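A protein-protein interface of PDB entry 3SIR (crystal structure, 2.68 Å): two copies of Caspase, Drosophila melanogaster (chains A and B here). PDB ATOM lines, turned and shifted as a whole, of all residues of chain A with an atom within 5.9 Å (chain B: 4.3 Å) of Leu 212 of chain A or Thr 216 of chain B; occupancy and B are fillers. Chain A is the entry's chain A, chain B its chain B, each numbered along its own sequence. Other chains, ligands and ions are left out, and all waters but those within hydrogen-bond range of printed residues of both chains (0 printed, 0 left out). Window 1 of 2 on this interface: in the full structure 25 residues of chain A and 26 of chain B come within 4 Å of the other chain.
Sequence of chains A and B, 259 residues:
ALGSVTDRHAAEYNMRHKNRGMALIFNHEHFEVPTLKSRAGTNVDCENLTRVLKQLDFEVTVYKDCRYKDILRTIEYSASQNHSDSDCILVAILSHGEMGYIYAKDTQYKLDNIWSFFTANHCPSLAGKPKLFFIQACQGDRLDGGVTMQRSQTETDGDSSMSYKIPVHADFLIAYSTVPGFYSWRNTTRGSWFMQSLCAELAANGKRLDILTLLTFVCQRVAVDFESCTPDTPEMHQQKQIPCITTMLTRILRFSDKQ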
ATOM      1  N   ASP A   7      -2.197   8.059 -17.642  1.00  0.00           N
ATOM      2  CA  ASP A   7      -2.705   7.110 -16.674  1.00  0.00           C
ATOM      3  C   ASP A   7      -3.317   7.986 -15.593  1.00  0.00           C
ATOM      4  O   ASP A   7      -3.097   9.198 -15.588  1.00  0.00           O
ATOM      5  CB  ASP A   7      -1.561   6.269 -16.112  1.00  0.00           C
ATOM      6  CG  ASP A   7      -0.282   6.400 -16.922  1.00  0.00           C
ATOM      7  OD1 ASP A   7       0.023   7.505 -17.420  1.00  0.00           O
ATOM      8  OD2 ASP A   7       0.478   5.414 -16.982  1.00  0.00           O
ATOM      9  N   LEU A 173      13.329   3.889  -6.982  1.00  0.00           N
ATOM     10  CA  LEU A 173      14.162   3.040  -7.831  1.00  0.00           C
ATOM     11  C   LEU A 173      15.522   2.770  -7.200  1.00  0.00           C
ATOM     12  O   LEU A 173      16.287   3.697  -6.941  1.00  0.00           O
ATOM     13  CB  LEU A 173      14.367   3.677  -9.207  1.00  0.00           C
ATOM     14  CG  LEU A 173      15.397   2.991 -10.109  1.00  0.00           C
ATOM     15  CD1 LEU A 173      15.180   3.352 -11.574  1.00  0.00           C
ATOM     16  CD2 LEU A 173      16.822   3.325  -9.680  1.00  0.00           C
ATOM     17  N   ASP A 210      15.251   8.338 -21.320  1.00  0.00           N
ATOM     18  CA  ASP A 210      14.519   8.119 -20.077  1.00  0.00           C
ATOM     19  C   ASP A 210      15.208   7.083 -19.192  1.00  0.00           C
ATOM     20  O   ASP A 210      15.890   6.186 -19.690  1.00  0.00           O
ATOM     21  CB  ASP A 210      13.066   7.721 -20.364  1.00  0.00           C
ATOM     22  CG  ASP A 210      12.879   6.221 -20.497  1.00  0.00           C
ATOM     23  OD1 ASP A 210      12.297   5.610 -19.574  1.00  0.00           O
ATOM     24  OD2 ASP A 210      13.262   5.660 -21.545  1.00  0.00           O
ATOM     25  N   ILE A 211      15.053   7.231 -17.880  1.00  0.00           N
ATOM     26  CA  ILE A 211      15.971   6.626 -16.922  1.00  0.00           C
ATOM     27  C   ILE A 211      16.166   5.125 -17.145  1.00  0.00           C
ATOM     28  O   ILE A 211      17.286   4.615 -17.053  1.00  0.00           O
ATOM     29  CB  ILE A 211      15.521   6.891 -15.475  1.00  0.00           C
ATOM     30  CG1 ILE A 211      16.589   6.429 -14.477  1.00  0.00           C
ATOM     31  CG2 ILE A 211      14.186   6.224 -15.201  1.00  0.00           C
ATOM     32  CD1 ILE A 211      17.841   7.285 -14.482  1.00  0.00           C
ATOM     33  N   LEU A 212      15.091   4.439 -17.524  1.00  0.00           N
ATOM     34  CA  LEU A 212      15.077   2.980 -17.522  1.00  0.00           C
ATOM     35  C   LEU A 212      15.748   2.389 -18.763  1.00  0.00           C
ATOM     36  O   LEU A 212      16.265   1.269 -18.728  1.00  0.00           O
ATOM     37  CB  LEU A 212      13.647   2.451 -17.393  1.00  0.00           C
ATOM     38  CG  LEU A 212      12.942   2.672 -16.054  1.00  0.00           C
ATOM     39  CD1 LEU A 212      11.467   2.312 -16.165  1.00  0.00           C
ATOM     40  CD2 LEU A 212      13.612   1.884 -14.937  1.00  0.00           C
ATOM     41  N   THR A 213      15.739   3.152 -19.853  1.00  0.00           N
ATOM     42  CA  THR A 213      16.512   2.805 -21.042  1.00  0.00           C
ATOM     43  C   THR A 213      17.952   3.304 -20.925  1.00  0.00           C
ATOM     44  O   THR A 213      18.865   2.759 -21.549  1.00  0.00           O
ATOM     45  CB  THR A 213      15.885   3.384 -22.326  1.00  0.00           C
ATOM     46  OG1 THR A 213      15.955   4.811 -22.282  1.00  0.00           O
ATOM     47  CG2 THR A 213      14.423   2.970 -22.464  1.00  0.00           C
ATOM     48  N   LEU A 214      18.176   4.283 -20.058  1.00  0.00           N
ATOM     49  CA  LEU A 214      19.525   4.540 -19.578  1.00  0.00           C
ATOM     50  C   LEU A 214      20.047   3.320 -18.818  1.00  0.00           C
ATOM     51  O   LEU A 214      20.871   2.565 -19.334  1.00  0.00           O
ATOM     52  CB  LEU A 214      19.545   5.777 -18.684  1.00  0.00           C
ATOM     53  CG  LEU A 214      20.759   6.698 -18.797  1.00  0.00           C
ATOM     54  CD1 LEU A 214      21.239   6.741 -20.233  1.00  0.00           C
ATOM     55  CD2 LEU A 214      20.402   8.099 -18.321  1.00  0.00           C
ATOM     56  N   LEU A 215      19.441   3.043 -17.667  1.00  0.00           N
ATOM     57  CA  LEU A 215      19.883   1.948 -16.799  1.00  0.00           C
ATOM     58  C   LEU A 215      19.719   0.574 -17.440  1.00  0.00           C
ATOM     59  O   LEU A 215      20.105  -0.441 -16.862  1.00  0.00           O
ATOM     60  CB  LEU A 215      19.137   1.979 -15.462  1.00  0.00           C
ATOM     61  CG  LEU A 215      19.157   3.313 -14.721  1.00  0.00           C
ATOM     62  CD1 LEU A 215      18.317   3.233 -13.459  1.00  0.00           C
ATOM     63  CD2 LEU A 215      20.593   3.694 -14.401  1.00  0.00           C
ATOM     64  N   THR A 216      19.081   0.538 -18.604  1.00  0.00           N
ATOM     65  CA  THR A 216      19.053  -0.676 -19.404  1.00  0.00           C
ATOM     66  C   THR A 216      20.374  -0.836 -20.143  1.00  0.00           C
ATOM     67  O   THR A 216      20.953  -1.924 -20.180  1.00  0.00           O
ATOM     68  CB  THR A 216      17.911  -0.640 -20.421  1.00  0.00           C
ATOM     69  OG1 THR A 216      16.669  -0.875 -19.744  1.00  0.00           O
ATOM     70  CG2 THR A 216      18.131  -1.705 -21.486  1.00  0.00           C
ATOM     71  N   PHE A 217      20.901   0.283 -20.625  1.00  0.00           N
ATOM     72  CA  PHE A 217      22.148   0.274 -21.370  1.00  0.00           C
ATOM     73  C   PHE A 217      23.353   0.188 -20.438  1.00  0.00           C
ATOM     74  O   PHE A 217      24.399  -0.351 -20.809  1.00  0.00           O
ATOM     75  CB  PHE A 217      22.238   1.511 -22.263  1.00  0.00           C
ATOM     76  CG  PHE A 217      21.160   1.581 -23.309  1.00  0.00           C
ATOM     77  CD1 PHE A 217      20.563   0.425 -23.781  1.00  0.00           C
ATOM     78  CD2 PHE A 217      20.804   2.794 -23.873  1.00  0.00           C
ATOM     79  CE1 PHE A 217      19.607   0.475 -24.783  1.00  0.00           C
ATOM     80  CE2 PHE A 217      19.862   2.855 -24.887  1.00  0.00           C
ATOM     81  CZ  PHE A 217      19.251   1.692 -25.334  1.00  0.00           C
ATOM     82  N   ILE A 245      18.296  -3.584 -11.454  1.00  0.00           N
ATOM     83  CA  ILE A 245      17.499  -2.385 -11.242  1.00  0.00           C
ATOM     84  C   ILE A 245      16.094  -2.773 -10.811  1.00  0.00           C
ATOM     85  O   ILE A 245      15.476  -3.646 -11.419  1.00  0.00           O
ATOM     86  CB  ILE A 245      17.423  -1.527 -12.510  1.00  0.00           C
ATOM     87  CG1 ILE A 245      18.798  -0.933 -12.827  1.00  0.00           C
ATOM     88  CG2 ILE A 245      16.383  -0.431 -12.340  1.00  0.00           C
ATOM     89  CD1 ILE A 245      19.209  -1.096 -14.274  1.00  0.00           C
ATOM     90  N   THR A 247      12.444  -1.045 -10.043  1.00  0.00           N
ATOM     91  CA  THR A 247      11.657   0.185 -10.090  1.00  0.00           C
ATOM     92  C   THR A 247      10.270   0.040  -9.476  1.00  0.00           C
ATOM     93  O   THR A 247       9.611  -0.987  -9.646  1.00  0.00           O
ATOM     94  CB  THR A 247      11.480   0.693 -11.518  1.00  0.00           C
ATOM     95  OG1 THR A 247      10.303   1.507 -11.566  1.00  0.00           O
ATOM     96  CG2 THR A 247      11.316  -0.477 -12.468  1.00  0.00           C
ATOM     97  N   LEU A 249       8.802   3.273 -10.153  1.00  0.00           N
ATOM     98  CA  LEU A 249       8.464   4.514 -10.830  1.00  0.00           C
ATOM     99  C   LEU A 249       7.055   4.385 -11.393  1.00  0.00           C
ATOM    100  O   LEU A 249       6.701   3.351 -11.946  1.00  0.00           O
ATOM    101  CB  LEU A 249       9.466   4.811 -11.945  1.00  0.00           C
ATOM    102  CG  LEU A 249      10.932   4.969 -11.537  1.00  0.00           C
ATOM    103  CD1 LEU A 249      11.686   5.734 -12.613  1.00  0.00           C
ATOM    104  CD2 LEU A 249      11.061   5.685 -10.203  1.00  0.00           C
ATOM    105  N   THR A 250       6.204   5.356 -11.087  1.00  0.00           N
ATOM    106  CA  THR A 250       4.876   5.402 -11.678  1.00  0.00           C
ATOM    107  C   THR A 250       4.856   6.139 -13.020  1.00  0.00           C
ATOM    108  O   THR A 250       3.826   6.154 -13.697  1.00  0.00           O
ATOM    109  CB  THR A 250       3.857   6.041 -10.715  1.00  0.00           C
ATOM    110  OG1 THR A 250       4.371   7.293 -10.245  1.00  0.00           O
ATOM    111  CG2 THR A 250       3.600   5.127  -9.524  1.00  0.00           C
ATOM    112  N   ARG A 251       6.013   6.648 -13.449  1.00  0.00           N
ATOM    113  CA  ARG A 251       6.091   7.533 -14.612  1.00  0.00           C
ATOM    114  C   ARG A 251       7.465   7.545 -15.277  1.00  0.00           C
ATOM    115  O   ARG A 251       8.478   7.255 -14.643  1.00  0.00           O
ATOM    116  CB  ARG A 251       5.697   8.964 -14.230  1.00  0.00           C
ATOM    117  CG  ARG A 251       4.741   9.067 -13.047  1.00  0.00           C
ATOM    118  CD  ARG A 251       3.808  10.260 -13.189  1.00  0.00           C
ATOM    119  NE  ARG A 251       3.571  10.926 -11.911  1.00  0.00           N
ATOM    120  CZ  ARG A 251       2.993  12.116 -11.783  1.00  0.00           C
ATOM    121  NH1 ARG A 251       2.533  12.748 -12.854  1.00  0.00           N
ATOM    122  NH2 ARG A 251       2.904  12.687 -10.587  1.00  0.00           N
ATOM    123  N   ILE A 252       7.505   8.028 -16.516  1.00  0.00           N
ATOM    124  CA  ILE A 252       8.747   8.174 -17.271  1.00  0.00           C
ATOM    125  C   ILE A 252       9.594   9.325 -16.746  1.00  0.00           C
ATOM    126  O   ILE A 252       9.240  10.496 -16.922  1.00  0.00           O
ATOM    127  CB  ILE A 252       8.452   8.475 -18.752  1.00  0.00           C
ATOM    128  CG1 ILE A 252       7.579   7.377 -19.358  1.00  0.00           C
ATOM    129  CG2 ILE A 252       9.738   8.669 -19.546  1.00  0.00           C
ATOM    130  CD1 ILE A 252       6.748   7.857 -20.523  1.00  0.00           C
ATOM    131  N   LEU A 253      10.792   8.996 -16.273  1.00  0.00           N
ATOM    132  CA  LEU A 253      11.695   9.999 -15.718  1.00  0.00           C
ATOM    133  C   LEU A 253      12.727  10.417 -16.761  1.00  0.00           C
ATOM    134  O   LEU A 253      13.445   9.580 -17.299  1.00  0.00           O
ATOM    135  CB  LEU A 253      12.380   9.452 -14.461  1.00  0.00           C
ATOM    136  CG  LEU A 253      13.614  10.155 -13.886  1.00  0.00           C
ATOM    137  CD1 LEU A 253      13.560  11.645 -14.136  1.00  0.00           C
ATOM    138  CD2 LEU A 253      13.716   9.882 -12.393  1.00  0.00           C
ATOM    139  N   LEU B 212       9.217  -1.795 -20.448  1.00  0.00           N
ATOM    140  CA  LEU B 212       9.665  -1.206 -19.193  1.00  0.00           C
ATOM    141  C   LEU B 212       8.932   0.091 -18.878  1.00  0.00           C
ATOM    142  O   LEU B 212       8.727   0.431 -17.709  1.00  0.00           O
ATOM    143  CB  LEU B 212      11.179  -0.991 -19.208  1.00  0.00           C
ATOM    144  CG  LEU B 212      11.962  -2.251 -18.845  1.00  0.00           C
ATOM    145  CD1 LEU B 212      13.440  -1.935 -18.722  1.00  0.00           C
ATOM    146  CD2 LEU B 212      11.423  -2.871 -17.555  1.00  0.00           C
ATOM    147  N   THR B 213       8.463   0.774 -19.917  1.00  0.00           N
ATOM    148  CA  THR B 213       7.480   1.829 -19.713  1.00  0.00           C
ATOM    149  C   THR B 213       6.068   1.255 -19.640  1.00  0.00           C
ATOM    150  O   THR B 213       5.308   1.602 -18.738  1.00  0.00           O
ATOM    151  CB  THR B 213       7.574   2.948 -20.769  1.00  0.00           C
ATOM    152  OG1 THR B 213       6.876   2.556 -21.958  1.00  0.00           O
ATOM    153  CG2 THR B 213       9.026   3.249 -21.105  1.00  0.00           C
ATOM    154  N   LEU B 214       5.786   0.245 -20.456  1.00  0.00           N
ATOM    155  CA  LEU B 214       4.526  -0.479 -20.319  1.00  0.00           C
ATOM    156  C   LEU B 214       4.286  -0.787 -18.849  1.00  0.00           C
ATOM    157  O   LEU B 214       3.265  -0.398 -18.281  1.00  0.00           O
ATOM    158  CB  LEU B 214       4.541  -1.782 -21.119  1.00  0.00           C
ATOM    159  CG  LEU B 214       3.168  -2.414 -21.386  1.00  0.00           C
ATOM    160  CD1 LEU B 214       2.288  -1.442 -22.152  1.00  0.00           C
ATOM    161  CD2 LEU B 214       3.284  -3.729 -22.153  1.00  0.00           C
ATOM    162  N   LEU B 215       5.275  -1.423 -18.228  1.00  0.00           N
ATOM    163  CA  LEU B 215       5.156  -1.876 -16.847  1.00  0.00           C
ATOM    164  C   LEU B 215       5.191  -0.707 -15.864  1.00  0.00           C
ATOM    165  O   LEU B 215       4.541  -0.748 -14.817  1.00  0.00           O
ATOM    166  CB  LEU B 215       6.263  -2.883 -16.513  1.00  0.00           C
ATOM    167  CG  LEU B 215       6.271  -4.216 -17.262  1.00  0.00           C
ATOM    168  CD1 LEU B 215       7.534  -5.002 -16.940  1.00  0.00           C
ATOM    169  CD2 LEU B 215       5.030  -5.043 -16.948  1.00  0.00           C
ATOM    170  N   THR B 216       5.973   0.322 -16.184  1.00  0.00           N
ATOM    171  CA  THR B 216       5.948   1.550 -15.395  1.00  0.00           C
ATOM    172  C   THR B 216       4.532   2.087 -15.228  1.00  0.00           C
ATOM    173  O   THR B 216       4.069   2.282 -14.104  1.00  0.00           O
ATOM    174  CB  THR B 216       6.817   2.648 -16.008  1.00  0.00           C
ATOM    175  OG1 THR B 216       8.186   2.422 -15.653  1.00  0.00           O
ATOM    176  CG2 THR B 216       6.391   3.999 -15.476  1.00  0.00           C
ATOM    177  N   PHE B 217       3.829   2.249 -16.346  1.00  0.00           N
ATOM    178  CA  PHE B 217       2.436   2.671 -16.328  1.00  0.00           C
ATOM    179  C   PHE B 217       1.554   1.635 -15.647  1.00  0.00           C
ATOM    180  O   PHE B 217       0.494   1.963 -15.112  1.00  0.00           O
ATOM    181  CB  PHE B 217       1.926   2.933 -17.747  1.00  0.00           C
ATOM    182  CG  PHE B 217       2.716   3.968 -18.499  1.00  0.00           C
ATOM    183  CD1 PHE B 217       3.297   5.040 -17.834  1.00  0.00           C
ATOM    184  CD2 PHE B 217       2.880   3.867 -19.870  1.00  0.00           C
ATOM    185  CE1 PHE B 217       4.034   5.990 -18.524  1.00  0.00           C
ATOM    186  CE2 PHE B 217       3.611   4.811 -20.570  1.00  0.00           C
ATOM    187  CZ  PHE B 217       4.186   5.876 -19.897  1.00  0.00           C
ATOM    188  N   VAL B 218       1.971   0.374 -15.675  1.00  0.00           N
ATOM    189  CA  VAL B 218       1.262  -0.626 -14.887  1.00  0.00           C
ATOM    190  C   VAL B 218       1.383  -0.316 -13.394  1.00  0.00           C
ATOM    191  O   VAL B 218       0.427  -0.494 -12.640  1.00  0.00           O
ATOM    192  CB  VAL B 218       1.731  -2.062 -15.209  1.00  0.00           C
ATOM    193  CG1 VAL B 218       1.057  -3.070 -14.290  1.00  0.00           C
ATOM    194  CG2 VAL B 218       1.438  -2.394 -16.667  1.00  0.00           C
ATOM    195  N   CYS B 219       2.508   0.275 -12.999  1.00  0.00           N
ATOM    196  CA  CYS B 219       2.700   0.721 -11.621  1.00  0.00           C
ATOM    197  C   CYS B 219       1.795   1.903 -11.307  1.00  0.00           C
ATOM    198  O   CYS B 219       1.267   2.015 -10.198  1.00  0.00           O
ATOM    199  CB  CYS B 219       4.157   1.124 -11.372  1.00  0.00           C
ATOM    200  SG  CYS B 219       5.376  -0.191 -11.611  1.00  0.00           S
ATOM    201  N   GLN B 220       1.703   2.833 -12.254  1.00  0.00           N
ATOM    202  CA  GLN B 220       0.974   4.075 -12.025  1.00  0.00           C
ATOM    203  C   GLN B 220      -0.526   3.824 -11.920  1.00  0.00           C
ATOM    204  O   GLN B 220      -1.215   4.468 -11.131  1.00  0.00           O
ATOM    205  CB  GLN B 220       1.269   5.104 -13.120  1.00  0.00           C
ATOM    206  CG  GLN B 220       0.861   6.527 -12.740  1.00  0.00           C
ATOM    207  CD  GLN B 220       0.703   7.452 -13.937  1.00  0.00           C
ATOM    208  OE1 GLN B 220       1.666   7.735 -14.653  1.00  0.00           O
ATOM    209  NE2 GLN B 220      -0.496   8.002 -14.099  1.00  0.00           N
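Leu 212 of chain B touches its own counterpart, Leu 212 of chain A.
Leu 212 of chain A touches Thr 216 of chain B, and with the chains exchanged Thr 216 of chain A touches Leu 212 of chain B.
Of the 13 pairs that touch across the chains among the printed residues, 3 have their exchanged pair printed and touching as well.
Printed residues of chain B within 4 Å of Asp 7 of chain A: Phe 217 (3.0 Å) and Gln 220 (2.9 Å).
Of chain B, only Leu 212 (3.7 Å) and Thr 216 (3.3 Å) come within 4 Å of Leu 212 of chain A.
Printed residues of chain B within 4 Å of Thr 216 of chain A: Leu 212 (3.5 Å).
Ile 245 of chain A touches none of the printed residues of chain B.
Of the printed residues of chain B, Ile 252 of chain A touches Phe 217.
Thr 216 of chain B touches four residues of chain A.
Of the printed residues of chain A, Phe 217 of chain B touches Asp 7 and Ile 252.
The nearest printed residue of chain B that does not touch Leu 212 of chain A is Thr 213 of chain B (5.0 Å).
The nearest residue of chain A that does not touch Thr 216 of chain B is Ile 252 of chain A (4.3 Å).
The nearest printed residue of chain B that does not touch Leu 249 of chain A is Gln 220 of chain B (5.0 Å).
Printed residues of chain B that touch a printed residue of chain A: Leu 212, Thr 216, Phe 217, Cys 219 and Gln 220.
Along chain B the printed residues that touch a printed residue of chain A span positions 212 to 220.
Hydrophobic or aromatic side chains of chain A that line the printed part of chain B: Leu 212 and Ile 252.
Among the printed residues, 13 pairs touch across the chains.
The side-chain carboxylate (OD1) of Asp 7 of chain A sits close to the side-chain amide oxygen (OE1) of Gln 220 of chain B (3.2 Å).
O of Leu 249 of chain A sits close to SG of Cys 219 of chain B, at 3.8 Å.
The side-chain amide oxygen (OE1) of Gln 220 of chain B lies close to the backbone carbonyl oxygen (O) of Thr 250 of chain A.
Asp 7 of chain A touches Phe 217 of chain B.
CD1 of Leu 212 of chain A touches O of Leu 212 of chain B, at 3.7 Å.
Thr 216 of chain B touches Leu 212 of chain A.
CD1 of Leu 212 of chain B touches OG1 of Thr 216 of chain A, 3.5 Å away.
Thr 216 of chain B touches Leu 249 of chain A (O to O, 3.6 Å).
C of Thr 250 of chain A touches CG2 of Thr 216 of chain B (3.6 Å).
Cys 219 of chain B touches Thr 250 of chain A.
Arg 251 of chain A touches Thr 216 of chain B (N to CG2, 3.4 Å).
CD of Arg 251 of chain A touches OE1 of Gln 220 of chain B, at 3.6 Å.
CD1 of Ile 252 of chain A touches CZ of Phe 217 of chain B, at 3.3 Å.
The backbone carbonyl oxygen (O) of Leu 212 of chain A lies within hydrogen-bond range of the side-chain hydroxyl (OG1) of Thr 216 of chain A (2.4 Å).
The backbone NH (N) of Leu 249 of chain A is in hydrogen-bond range of the side-chain hydroxyl (OG1) of Thr 247 of chain A (2.7 Å).
The side-chain hydroxyl of Thr 216 of chain B sits at hydrogen-bond distance from the backbone carbonyl oxygen of Leu 212 of chain B.
O of Leu 215 of chain B lies within hydrogen-bond range of SG of Cys 219 of chain B (3.4 Å).
The side-chain sulfur (SG) of Cys 219 of chain B lies close to the backbone carbonyl oxygen (O) of Thr 216 of chain B.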
